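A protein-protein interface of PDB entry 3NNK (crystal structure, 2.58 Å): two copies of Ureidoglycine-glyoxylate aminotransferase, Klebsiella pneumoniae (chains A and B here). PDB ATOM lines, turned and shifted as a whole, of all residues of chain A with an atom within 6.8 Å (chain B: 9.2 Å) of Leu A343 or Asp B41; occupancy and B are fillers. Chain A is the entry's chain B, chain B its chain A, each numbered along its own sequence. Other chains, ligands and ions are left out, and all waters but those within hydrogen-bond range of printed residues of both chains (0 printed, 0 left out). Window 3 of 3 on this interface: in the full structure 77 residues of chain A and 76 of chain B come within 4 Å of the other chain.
The side-chain carboxylate (OD2) of Asp B41 lies within salt-bridge range of the guanidinium group (NE) of Arg A14 (2.6 Å).
The backbone NH of Ala B43 lies close to the side-chain carboxylate of Asp B41 (3.2 Å).
The backbone NH of Glu A349 lies within hydrogen-bond range of the backbone carbonyl oxygen of Leu A15, at 2.9 Å.
N of Leu A343 is in hydrogen-bond range of O of Ile A348 (3.2 Å).
Among the printed residues, merely in contact across the chains: Glu A349 with Gly B38 (3.3 Å), Leu A16 with Gly B38 (3.4 Å), Leu A343 with Asp B41 (3.5 Å), Leu A16 with Ile B37 (3.7 Å), Pro A12 with Ile B37 (3.7 Å), Pro A12 with Ala B43 (3.7 Å) and Arg A14 with Ile B37 (3.8 Å).
Of the printed residues of chain B, Arg A14 touches Ile B37 and Asp B41.
Of the printed residues of chain B, Leu A16 touches Ile B37 (3.7 Å) and Gly B38 (3.4 Å).
Of chain B, only Asp B41 comes within 4 Å of Leu A343.
No residue of chain B comes within 4 Å of Gly A347.
Printed residues of chain A within 4 Å of Ile B37: Pro A12, Arg A14 and Leu A16.
Of the printed residues of chain A, Gly B38 touches Leu A16 (3.4 Å) and Glu A349 (3.3 Å).
Asp B41 touches two residues of chain A.
Met B44 touches none of the printed residues of chain A.
The nearest residue of chain B that does not touch Leu A343 is Pro B42 (4.1 Å).
The nearest residue of chain A that does not touch Asp B41 is Pro A12 (4.1 Å).
Of the 18 printed residues of chain A, 5 touch a printed residue of chain B.
Printed residues of chain A that touch a printed residue of chain B: Pro A12, Arg A14, Leu A16, Leu A343 and Glu A349.
Hydrophobic or aromatic side chains of chain A that line the printed part of chain B: Pro A12, Leu A16 and Leu A343.
Hydrophobic or aromatic side chains of chain B that line the printed part of chain A: Ile B37 and Ala B43.
Among the printed residues, Asp or Glu carboxylates within 4 Å of a Lys or Arg side-chain nitrogen of the other chain: Arg A14 with Asp B41 (2.6 Å).
No position is printed for both chains.
Of the 8 pairs that touch across the chains among the printed residues, none has its exchanged pair printed and touching as well.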
ATOM      1  N   PRO A  12      -8.232 -20.804  -7.804  1.00  0.00           N
ATOM      2  CA  PRO A  12      -8.480 -21.771  -8.869  1.00  0.00           C
ATOM      3  C   PRO A  12      -9.717 -22.613  -8.578  1.00  0.00           C
ATOM      4  O   PRO A  12     -10.078 -22.795  -7.412  1.00  0.00           O
ATOM      5  CB  PRO A  12      -7.221 -22.641  -8.854  1.00  0.00           C
ATOM      6  CG  PRO A  12      -6.706 -22.546  -7.460  1.00  0.00           C
ATOM      7  CD  PRO A  12      -7.079 -21.180  -6.962  1.00  0.00           C
ATOM      8  N   SER A  13     -10.363 -23.106  -9.631  1.00  0.00           N
ATOM      9  CA  SER A  13     -11.526 -23.978  -9.488  1.00  0.00           C
ATOM     10  C   SER A  13     -11.119 -25.299  -8.839  1.00  0.00           C
ATOM     11  O   SER A  13     -10.183 -25.964  -9.293  1.00  0.00           O
ATOM     12  CB  SER A  13     -12.185 -24.229 -10.846  1.00  0.00           C
ATOM     13  OG  SER A  13     -13.397 -24.951 -10.698  1.00  0.00           O
ATOM     14  N   ARG A  14     -11.815 -25.662  -7.765  1.00  0.00           N
ATOM     15  CA  ARG A  14     -11.496 -26.865  -7.005  1.00  0.00           C
ATOM     16  C   ARG A  14     -12.752 -27.642  -6.645  1.00  0.00           C
ATOM     17  O   ARG A  14     -13.725 -27.062  -6.160  1.00  0.00           O
ATOM     18  CB  ARG A  14     -10.750 -26.500  -5.714  1.00  0.00           C
ATOM     19  CG  ARG A  14      -9.373 -25.875  -5.903  1.00  0.00           C
ATOM     20  CD  ARG A  14      -8.296 -26.930  -6.059  1.00  0.00           C
ATOM     21  NE  ARG A  14      -6.969 -26.344  -6.231  1.00  0.00           N
ATOM     22  CZ  ARG A  14      -6.315 -26.283  -7.388  1.00  0.00           C
ATOM     23  NH1 ARG A  14      -6.857 -26.775  -8.496  1.00  0.00           N
ATOM     24  NH2 ARG A  14      -5.110 -25.729  -7.435  1.00  0.00           N
ATOM     25  N   LEU A  15     -12.735 -28.949  -6.888  1.00  0.00           N
ATOM     26  CA  LEU A  15     -13.754 -29.827  -6.325  1.00  0.00           C
ATOM     27  C   LEU A  15     -13.222 -30.403  -5.014  1.00  0.00           C
ATOM     28  O   LEU A  15     -12.399 -31.323  -5.012  1.00  0.00           O
ATOM     29  CB  LEU A  15     -14.161 -30.939  -7.299  1.00  0.00           C
ATOM     30  CG  LEU A  15     -15.354 -31.802  -6.858  1.00  0.00           C
ATOM     31  CD1 LEU A  15     -16.664 -31.018  -6.920  1.00  0.00           C
ATOM     32  CD2 LEU A  15     -15.452 -33.078  -7.682  1.00  0.00           C
ATOM     33  N   LEU A  16     -13.691 -29.844  -3.903  1.00  0.00           N
ATOM     34  CA  LEU A  16     -13.210 -30.230  -2.583  1.00  0.00           C
ATOM     35  C   LEU A  16     -13.952 -31.451  -2.046  1.00  0.00           C
ATOM     36  O   LEU A  16     -15.100 -31.360  -1.598  1.00  0.00           O
ATOM     37  CB  LEU A  16     -13.285 -29.047  -1.605  1.00  0.00           C
ATOM     38  CG  LEU A  16     -12.538 -27.760  -1.994  1.00  0.00           C
ATOM     39  CD1 LEU A  16     -12.782 -26.652  -0.981  1.00  0.00           C
ATOM     40  CD2 LEU A  16     -11.041 -28.000  -2.176  1.00  0.00           C
ATOM     41  N   ALA A 338      -0.856 -39.482  -5.360  1.00  0.00           N
ATOM     42  CA  ALA A 338      -2.215 -39.523  -5.890  1.00  0.00           C
ATOM     43  C   ALA A 338      -2.916 -38.189  -5.641  1.00  0.00           C
ATOM     44  O   ALA A 338      -3.621 -37.687  -6.512  1.00  0.00           O
ATOM     45  CB  ALA A 338      -3.000 -40.673  -5.279  1.00  0.00           C
ATOM     46  N   ARG A 339      -2.697 -37.619  -4.454  1.00  0.00           N
ATOM     47  CA  ARG A 339      -3.228 -36.301  -4.093  1.00  0.00           C
ATOM     48  C   ARG A 339      -2.752 -35.191  -5.026  1.00  0.00           C
ATOM     49  O   ARG A 339      -3.562 -34.393  -5.499  1.00  0.00           O
ATOM     50  CB  ARG A 339      -2.888 -35.957  -2.638  1.00  0.00           C
ATOM     51  CG  ARG A 339      -3.967 -36.352  -1.644  1.00  0.00           C
ATOM     52  CD  ARG A 339      -3.514 -36.197  -0.194  1.00  0.00           C
ATOM     53  NE  ARG A 339      -3.094 -34.834   0.144  1.00  0.00           N
ATOM     54  CZ  ARG A 339      -1.861 -34.492   0.509  1.00  0.00           C
ATOM     55  NH1 ARG A 339      -0.903 -35.409   0.599  1.00  0.00           N
ATOM     56  NH2 ARG A 339      -1.582 -33.226   0.792  1.00  0.00           N
ATOM     57  N   LYS A 340      -1.446 -35.147  -5.288  1.00  0.00           N
ATOM     58  CA  LYS A 340      -0.869 -34.176  -6.223  1.00  0.00           C
ATOM     59  C   LYS A 340      -1.515 -34.280  -7.608  1.00  0.00           C
ATOM     60  O   LYS A 340      -1.902 -33.268  -8.193  1.00  0.00           O
ATOM     61  CB  LYS A 340       0.653 -34.345  -6.324  1.00  0.00           C
ATOM     62  CG  LYS A 340       1.308 -33.459  -7.383  1.00  0.00           C
ATOM     63  CD  LYS A 340       2.821 -33.610  -7.414  1.00  0.00           C
ATOM     64  CE  LYS A 340       3.423 -32.739  -8.509  1.00  0.00           C
ATOM     65  NZ  LYS A 340       4.903 -32.611  -8.387  1.00  0.00           N
ATOM     66  N   LEU A 341      -1.637 -35.505  -8.115  1.00  0.00           N
ATOM     67  CA  LEU A 341      -2.235 -35.749  -9.427  1.00  0.00           C
ATOM     68  C   LEU A 341      -3.742 -35.472  -9.460  1.00  0.00           C
ATOM     69  O   LEU A 341      -4.266 -35.005 -10.474  1.00  0.00           O
ATOM     70  CB  LEU A 341      -1.930 -37.174  -9.908  1.00  0.00           C
ATOM     71  CG  LEU A 341      -0.474 -37.498 -10.270  1.00  0.00           C
ATOM     72  CD1 LEU A 341      -0.282 -38.994 -10.407  1.00  0.00           C
ATOM     73  CD2 LEU A 341      -0.027 -36.790 -11.544  1.00  0.00           C
ATOM     74  N   MET A 342      -4.428 -35.753  -8.353  1.00  0.00           N
ATOM     75  CA  MET A 342      -5.861 -35.474  -8.227  1.00  0.00           C
ATOM     76  C   MET A 342      -6.162 -33.975  -8.227  1.00  0.00           C
ATOM     77  O   MET A 342      -7.162 -33.537  -8.797  1.00  0.00           O
ATOM     78  CB  MET A 342      -6.433 -36.104  -6.949  1.00  0.00           C
ATOM     79  CG  MET A 342      -6.591 -37.618  -6.990  1.00  0.00           C
ATOM     80  SD  MET A 342      -7.947 -38.186  -8.028  1.00  0.00           S
ATOM     81  CE  MET A 342      -9.355 -37.911  -6.952  1.00  0.00           C
ATOM     82  N   LEU A 343      -5.299 -33.200  -7.576  1.00  0.00           N
ATOM     83  CA  LEU A 343      -5.506 -31.765  -7.421  1.00  0.00           C
ATOM     84  C   LEU A 343      -5.023 -30.974  -8.635  1.00  0.00           C
ATOM     85  O   LEU A 343      -5.734 -30.106  -9.141  1.00  0.00           O
ATOM     86  CB  LEU A 343      -4.808 -31.263  -6.151  1.00  0.00           C
ATOM     87  CG  LEU A 343      -5.087 -29.830  -5.688  1.00  0.00           C
ATOM     88  CD1 LEU A 343      -6.308 -29.786  -4.782  1.00  0.00           C
ATOM     89  CD2 LEU A 343      -3.871 -29.262  -4.973  1.00  0.00           C
ATOM     90  N   GLU A 344      -3.813 -31.278  -9.096  1.00  0.00           N
ATOM     91  CA  GLU A 344      -3.182 -30.515 -10.171  1.00  0.00           C
ATOM     92  C   GLU A 344      -3.705 -30.871 -11.562  1.00  0.00           C
ATOM     93  O   GLU A 344      -3.815 -29.997 -12.427  1.00  0.00           O
ATOM     94  CB  GLU A 344      -1.656 -30.660 -10.118  1.00  0.00           C
ATOM     95  CG  GLU A 344      -1.010 -30.030  -8.880  1.00  0.00           C
ATOM     96  CD  GLU A 344       0.516 -30.096  -8.888  1.00  0.00           C
ATOM     97  OE1 GLU A 344       1.122 -30.071  -9.984  1.00  0.00           O
ATOM     98  OE2 GLU A 344       1.113 -30.162  -7.791  1.00  0.00           O
ATOM     99  N   ASP A 345      -4.032 -32.146 -11.770  1.00  0.00           N
ATOM    100  CA  ASP A 345      -4.445 -32.636 -13.090  1.00  0.00           C
ATOM    101  C   ASP A 345      -5.960 -32.780 -13.260  1.00  0.00           C
ATOM    102  O   ASP A 345      -6.453 -32.781 -14.387  1.00  0.00           O
ATOM    103  CB  ASP A 345      -3.750 -33.963 -13.425  1.00  0.00           C
ATOM    104  CG  ASP A 345      -2.233 -33.835 -13.511  1.00  0.00           C
ATOM    105  OD1 ASP A 345      -1.697 -32.719 -13.339  1.00  0.00           O
ATOM    106  OD2 ASP A 345      -1.569 -34.866 -13.753  1.00  0.00           O
ATOM    107  N   PHE A 346      -6.684 -32.905 -12.149  1.00  0.00           N
ATOM    108  CA  PHE A 346      -8.142 -33.050 -12.183  1.00  0.00           C
ATOM    109  C   PHE A 346      -8.867 -31.925 -11.448  1.00  0.00           C
ATOM    110  O   PHE A 346     -10.071 -31.733 -11.632  1.00  0.00           O
ATOM    111  CB  PHE A 346      -8.568 -34.402 -11.607  1.00  0.00           C
ATOM    112  CG  PHE A 346      -8.268 -35.568 -12.502  1.00  0.00           C
ATOM    113  CD1 PHE A 346      -9.239 -36.066 -13.362  1.00  0.00           C
ATOM    114  CD2 PHE A 346      -7.016 -36.175 -12.480  1.00  0.00           C
ATOM    115  CE1 PHE A 346      -8.968 -37.150 -14.190  1.00  0.00           C
ATOM    116  CE2 PHE A 346      -6.736 -37.255 -13.307  1.00  0.00           C
ATOM    117  CZ  PHE A 346      -7.712 -37.745 -14.160  1.00  0.00           C
ATOM    118  N   GLY A 347      -8.130 -31.183 -10.624  1.00  0.00           N
ATOM    119  CA  GLY A 347      -8.700 -30.088  -9.839  1.00  0.00           C
ATOM    120  C   GLY A 347      -9.581 -30.581  -8.708  1.00  0.00           C
ATOM    121  O   GLY A 347     -10.538 -29.906  -8.321  1.00  0.00           O
ATOM    122  N   ILE A 348      -9.255 -31.759  -8.180  1.00  0.00           N
ATOM    123  CA  ILE A 348     -10.044 -32.397  -7.129  1.00  0.00           C
ATOM    124  C   ILE A 348      -9.186 -32.644  -5.893  1.00  0.00           C
ATOM    125  O   ILE A 348      -8.116 -33.250  -5.978  1.00  0.00           O
ATOM    126  CB  ILE A 348     -10.671 -33.733  -7.612  1.00  0.00           C
ATOM    127  CG1 ILE A 348     -11.546 -33.501  -8.847  1.00  0.00           C
ATOM    128  CG2 ILE A 348     -11.483 -34.397  -6.493  1.00  0.00           C
ATOM    129  CD1 ILE A 348     -11.796 -34.743  -9.675  1.00  0.00           C
ATOM    130  N   GLU A 349      -9.661 -32.165  -4.747  1.00  0.00           N
ATOM    131  CA  GLU A 349      -8.989 -32.418  -3.480  1.00  0.00           C
ATOM    132  C   GLU A 349      -9.582 -33.635  -2.780  1.00  0.00           C
ATOM    133  O   GLU A 349     -10.786 -33.702  -2.551  1.00  0.00           O
ATOM    134  CB  GLU A 349      -9.071 -31.195  -2.561  1.00  0.00           C
ATOM    135  CG  GLU A 349      -8.619 -31.470  -1.125  1.00  0.00           C
ATOM    136  CD  GLU A 349      -8.554 -30.223  -0.270  1.00  0.00           C
ATOM    137  OE1 GLU A 349      -7.702 -29.352  -0.553  1.00  0.00           O
ATOM    138  OE2 GLU A 349      -9.342 -30.122   0.696  1.00  0.00           O
ATOM    139  N   ILE A 350      -8.725 -34.599  -2.462  1.00  0.00           N
ATOM    140  CA  ILE A 350      -9.074 -35.657  -1.516  1.00  0.00           C
ATOM    141  C   ILE A 350      -8.191 -35.508  -0.280  1.00  0.00           C
ATOM    142  O   ILE A 350      -7.070 -35.005  -0.366  1.00  0.00           O
ATOM    143  CB  ILE A 350      -8.977 -37.087  -2.124  1.00  0.00           C
ATOM    144  CG1 ILE A 350      -7.566 -37.378  -2.652  1.00  0.00           C
ATOM    145  CG2 ILE A 350     -10.044 -37.278  -3.208  1.00  0.00           C
ATOM    146  CD1 ILE A 350      -7.273 -38.854  -2.868  1.00  0.00           C
ATOM    147  N   LEU B  36     -14.177 -20.983  -2.842  1.00  0.00           N
ATOM    148  CA  LEU B  36     -13.174 -21.358  -1.843  1.00  0.00           C
ATOM    149  C   LEU B  36     -12.205 -22.432  -2.341  1.00  0.00           C
ATOM    150  O   LEU B  36     -12.429 -23.053  -3.383  1.00  0.00           O
ATOM    151  CB  LEU B  36     -13.857 -21.853  -0.559  1.00  0.00           C
ATOM    152  CG  LEU B  36     -15.139 -21.200  -0.029  1.00  0.00           C
ATOM    153  CD1 LEU B  36     -15.693 -22.018   1.130  1.00  0.00           C
ATOM    154  CD2 LEU B  36     -14.926 -19.747   0.393  1.00  0.00           C
ATOM    155  N   ILE B  37     -11.126 -22.632  -1.585  1.00  0.00           N
ATOM    156  CA  ILE B  37     -10.182 -23.735  -1.808  1.00  0.00           C
ATOM    157  C   ILE B  37      -9.882 -24.469  -0.498  1.00  0.00           C
ATOM    158  O   ILE B  37     -10.266 -24.008   0.582  1.00  0.00           O
ATOM    159  CB  ILE B  37      -8.840 -23.274  -2.476  1.00  0.00           C
ATOM    160  CG1 ILE B  37      -8.007 -22.378  -1.537  1.00  0.00           C
ATOM    161  CG2 ILE B  37      -9.086 -22.658  -3.866  1.00  0.00           C
ATOM    162  CD1 ILE B  37      -8.401 -20.896  -1.489  1.00  0.00           C
ATOM    163  N   GLY B  38      -9.196 -25.606  -0.603  1.00  0.00           N
ATOM    164  CA  GLY B  38      -8.823 -26.414   0.557  1.00  0.00           C
ATOM    165  C   GLY B  38      -7.852 -25.704   1.483  1.00  0.00           C
ATOM    166  O   GLY B  38      -7.121 -24.809   1.058  1.00  0.00           O
ATOM    167  N   GLN B  39      -7.847 -26.115   2.750  1.00  0.00           N
ATOM    168  CA  GLN B  39      -7.024 -25.489   3.790  1.00  0.00           C
ATOM    169  C   GLN B  39      -5.554 -25.296   3.391  1.00  0.00           C
ATOM    170  O   GLN B  39      -4.979 -24.234   3.639  1.00  0.00           O
ATOM    171  CB  GLN B  39      -7.125 -26.279   5.103  1.00  0.00           C
ATOM    172  CG  GLN B  39      -6.308 -25.688   6.244  1.00  0.00           C
ATOM    173  CD  GLN B  39      -6.620 -26.291   7.600  1.00  0.00           C
ATOM    174  OE1 GLN B  39      -6.560 -25.600   8.614  1.00  0.00           O
ATOM    175  NE2 GLN B  39      -6.950 -27.581   7.630  1.00  0.00           N
ATOM    176  N   TYR B  40      -4.964 -26.317   2.772  1.00  0.00           N
ATOM    177  CA  TYR B  40      -3.548 -26.288   2.398  1.00  0.00           C
ATOM    178  C   TYR B  40      -3.302 -26.321   0.890  1.00  0.00           C
ATOM    179  O   TYR B  40      -2.262 -26.803   0.432  1.00  0.00           O
ATOM    180  CB  TYR B  40      -2.789 -27.428   3.084  1.00  0.00           C
ATOM    181  CG  TYR B  40      -2.778 -27.321   4.588  1.00  0.00           C
ATOM    182  CD1 TYR B  40      -1.979 -26.378   5.232  1.00  0.00           C
ATOM    183  CD2 TYR B  40      -3.570 -28.160   5.369  1.00  0.00           C
ATOM    184  CE1 TYR B  40      -1.967 -26.272   6.611  1.00  0.00           C
ATOM    185  CE2 TYR B  40      -3.564 -28.064   6.753  1.00  0.00           C
ATOM    186  CZ  TYR B  40      -2.758 -27.116   7.365  1.00  0.00           C
ATOM    187  OH  TYR B  40      -2.741 -27.008   8.735  1.00  0.00           O
ATOM    188  N   ASP B  41      -4.261 -25.811   0.123  1.00  0.00           N
ATOM    189  CA  ASP B  41      -4.067 -25.634  -1.307  1.00  0.00           C
ATOM    190  C   ASP B  41      -2.939 -24.624  -1.505  1.00  0.00           C
ATOM    191  O   ASP B  41      -2.922 -23.590  -0.837  1.00  0.00           O
ATOM    192  CB  ASP B  41      -5.350 -25.130  -1.965  1.00  0.00           C
ATOM    193  CG  ASP B  41      -5.303 -25.223  -3.474  1.00  0.00           C
ATOM    194  OD1 ASP B  41      -4.986 -24.206  -4.123  1.00  0.00           O
ATOM    195  OD2 ASP B  41      -5.566 -26.319  -4.011  1.00  0.00           O
ATOM    196  N   PRO B  42      -1.980 -24.928  -2.402  1.00  0.00           N
ATOM    197  CA  PRO B  42      -0.872 -24.013  -2.684  1.00  0.00           C
ATOM    198  C   PRO B  42      -1.309 -22.552  -2.839  1.00  0.00           C
ATOM    199  O   PRO B  42      -0.574 -21.647  -2.440  1.00  0.00           O
ATOM    200  CB  PRO B  42      -0.312 -24.551  -4.000  1.00  0.00           C
ATOM    201  CG  PRO B  42      -0.553 -26.018  -3.915  1.00  0.00           C
ATOM    202  CD  PRO B  42      -1.840 -26.196  -3.145  1.00  0.00           C
ATOM    203  N   ALA B  43      -2.497 -22.336  -3.401  1.00  0.00           N
ATOM    204  CA  ALA B  43      -3.064 -20.996  -3.560  1.00  0.00           C
ATOM    205  C   ALA B  43      -3.473 -20.355  -2.230  1.00  0.00           C
ATOM    206  O   ALA B  43      -3.359 -19.140  -2.068  1.00  0.00           O
ATOM    207  CB  ALA B  43      -4.242 -21.029  -4.519  1.00  0.00           C
ATOM    208  N   MET B  44      -3.949 -21.171  -1.290  1.00  0.00           N
ATOM    209  CA  MET B  44      -4.393 -20.681   0.019  1.00  0.00           C
ATOM    210  C   MET B  44      -3.222 -20.284   0.920  1.00  0.00           C
ATOM    211  O   MET B  44      -3.255 -19.223   1.549  1.00  0.00           O
ATOM    212  CB  MET B  44      -5.285 -21.714   0.717  1.00  0.00           C
ATOM    213  CG  MET B  44      -5.781 -21.311   2.107  1.00  0.00           C
ATOM    214  SD  MET B  44      -6.912 -19.900   2.118  1.00  0.00           S
ATOM    215  CE  MET B  44      -7.444 -19.932   3.831  1.00  0.00           C
ATOM    216  N   THR B  45      -2.197 -21.133   0.985  1.00  0.00           N
ATOM    217  CA  THR B  45      -0.990 -20.813   1.750  1.00  0.00           C
ATOM    218  C   THR B  45      -0.258 -19.634   1.117  1.00  0.00           C
ATOM    219  O   THR B  45       0.441 -18.886   1.804  1.00  0.00           O
ATOM    220  CB  THR B  45      -0.032 -22.021   1.895  1.00  0.00           C
ATOM    221  OG1 THR B  45       0.277 -22.557   0.602  1.00  0.00           O
ATOM    222  CG2 THR B  45      -0.655 -23.107   2.767  1.00  0.00           C
ATOM    223  N   HIS B  46      -0.433 -19.470  -0.193  1.00  0.00           N
ATOM    224  CA  HIS B  46       0.081 -18.304  -0.900  1.00  0.00           C
ATOM    225  C   HIS B  46      -0.629 -17.018  -0.473  1.00  0.00           C
ATOM    226  O   HIS B  46       0.028 -16.029  -0.141  1.00  0.00           O
ATOM    227  CB  HIS B  46      -0.024 -18.483  -2.416  1.00  0.00           C
ATOM    228  CG  HIS B  46       0.463 -17.298  -3.190  1.00  0.00           C
ATOM    229  ND1 HIS B  46      -0.386 -16.335  -3.688  1.00  0.00           N
ATOM    230  CD2 HIS B  46       1.715 -16.908  -3.524  1.00  0.00           C
ATOM    231  CE1 HIS B  46       0.321 -15.409  -4.312  1.00  0.00           C
ATOM    232  NE2 HIS B  46       1.598 -15.733  -4.228  1.00  0.00           N
ATOM    233  N   TYR B  47      -1.963 -17.032  -0.483  1.00  0.00           N
ATOM    234  CA  TYR B  47      -2.742 -15.848  -0.110  1.00  0.00           C
ATOM    235  C   TYR B  47      -2.515 -15.437   1.344  1.00  0.00           C
ATOM    236  O   TYR B  47      -2.478 -14.246   1.651  1.00  0.00           O
ATOM    237  CB  TYR B  47      -4.237 -16.037  -0.398  1.00  0.00           C
ATOM    238  CG  TYR B  47      -4.630 -15.822  -1.849  1.00  0.00           C
ATOM    239  CD1 TYR B  47      -5.421 -16.754  -2.520  1.00  0.00           C
ATOM    240  CD2 TYR B  47      -4.208 -14.691  -2.549  1.00  0.00           C
ATOM    241  CE1 TYR B  47      -5.785 -16.565  -3.847  1.00  0.00           C
ATOM    242  CE2 TYR B  47      -4.567 -14.493  -3.881  1.00  0.00           C
ATOM    243  CZ  TYR B  47      -5.355 -15.434  -4.522  1.00  0.00           C
ATOM    244  OH  TYR B  47      -5.716 -15.250  -5.839  1.00  0.00           O
ATOM    245  N   MET B  48      -2.355 -16.428   2.223  1.00  0.00           N
ATOM    246  CA  MET B  48      -1.987 -16.186   3.619  1.00  0.00           C
ATOM    247  C   MET B  48      -0.676 -15.409   3.713  1.00  0.00           C
ATOM    248  O   MET B  48      -0.557 -14.490   4.521  1.00  0.00           O
ATOM    249  CB  MET B  48      -1.868 -17.504   4.390  1.00  0.00           C
ATOM    250  CG  MET B  48      -3.193 -18.180   4.714  1.00  0.00           C
ATOM    251  SD  MET B  48      -2.979 -19.793   5.496  1.00  0.00           S
ATOM    252  CE  MET B  48      -2.642 -19.319   7.195  1.00  0.00           C
ATOM    253  N   ASN B  49       0.296 -15.787   2.881  1.00  0.00           N
ATOM    254  CA  ASN B  49       1.588 -15.098   2.802  1.00  0.00           C
ATOM    255  C   ASN B  49       1.465 -13.682   2.252  1.00  0.00           C
ATOM    256  O   ASN B  49       2.178 -12.777   2.693  1.00  0.00           O
ATOM    257  CB  ASN B  49       2.584 -15.894   1.951  1.00  0.00           C
ATOM    258  CG  ASN B  49       3.052 -17.172   2.625  1.00  0.00           C
ATOM    259  OD1 ASN B  49       3.564 -18.075   1.965  1.00  0.00           O
ATOM    260  ND2 ASN B  49       2.886 -17.254   3.941  1.00  0.00           N
ATOM    261  N   TYR B 257       0.797 -21.996  12.667  1.00  0.00           N
ATOM    262  CA  TYR B 257      -0.115 -22.243  11.547  1.00  0.00           C
ATOM    263  C   TYR B 257       0.239 -21.371  10.341  1.00  0.00           C
ATOM    264  O   TYR B 257       0.271 -21.857   9.209  1.00  0.00           O
ATOM    265  CB  TYR B 257      -1.571 -22.018  11.987  1.00  0.00           C
ATOM    266  CG  TYR B 257      -2.631 -22.261  10.925  1.00  0.00           C
ATOM    267  CD1 TYR B 257      -2.568 -23.365  10.072  1.00  0.00           C
ATOM    268  CD2 TYR B 257      -3.721 -21.400  10.801  1.00  0.00           C
ATOM    269  CE1 TYR B 257      -3.550 -23.589   9.106  1.00  0.00           C
ATOM    270  CE2 TYR B 257      -4.709 -21.616   9.841  1.00  0.00           C
ATOM    271  CZ  TYR B 257      -4.617 -22.713   8.999  1.00  0.00           C
ATOM    272  OH  TYR B 257      -5.592 -22.929   8.052  1.00  0.00           O
ATOM    273  N   ARG B 262       3.064 -25.026   9.148  1.00  0.00           N
ATOM    274  CA  ARG B 262       1.637 -25.118   8.786  1.00  0.00           C
ATOM    275  C   ARG B 262       0.823 -25.989   9.756  1.00  0.00           C
ATOM    276  O   ARG B 262      -0.158 -26.631   9.369  1.00  0.00           O
ATOM    277  CB  ARG B 262       1.462 -25.588   7.329  1.00  0.00           C
ATOM    278  CG  ARG B 262       2.055 -24.654   6.275  1.00  0.00           C
ATOM    279  CD  ARG B 262       1.326 -23.323   6.236  1.00  0.00           C
ATOM    280  NE  ARG B 262       1.881 -22.408   5.243  1.00  0.00           N
ATOM    281  CZ  ARG B 262       1.677 -21.094   5.243  1.00  0.00           C
ATOM    282  NH1 ARG B 262       0.937 -20.538   6.195  1.00  0.00           N
ATOM    283  NH2 ARG B 262       2.216 -20.334   4.298  1.00  0.00           N
ATOM    284  N   THR B 270     -11.728 -18.551   5.155  1.00  0.00           N
ATOM    285  CA  THR B 270     -11.374 -18.295   3.755  1.00  0.00           C
ATOM    286  C   THR B 270     -11.959 -16.979   3.241  1.00  0.00           C
ATOM    287  O   THR B 270     -11.230 -16.130   2.725  1.00  0.00           O
ATOM    288  CB  THR B 270     -11.816 -19.464   2.835  1.00  0.00           C
ATOM    289  OG1 THR B 270     -11.551 -20.714   3.482  1.00  0.00           O
ATOM    290  CG2 THR B 270     -11.071 -19.422   1.509  1.00  0.00           C
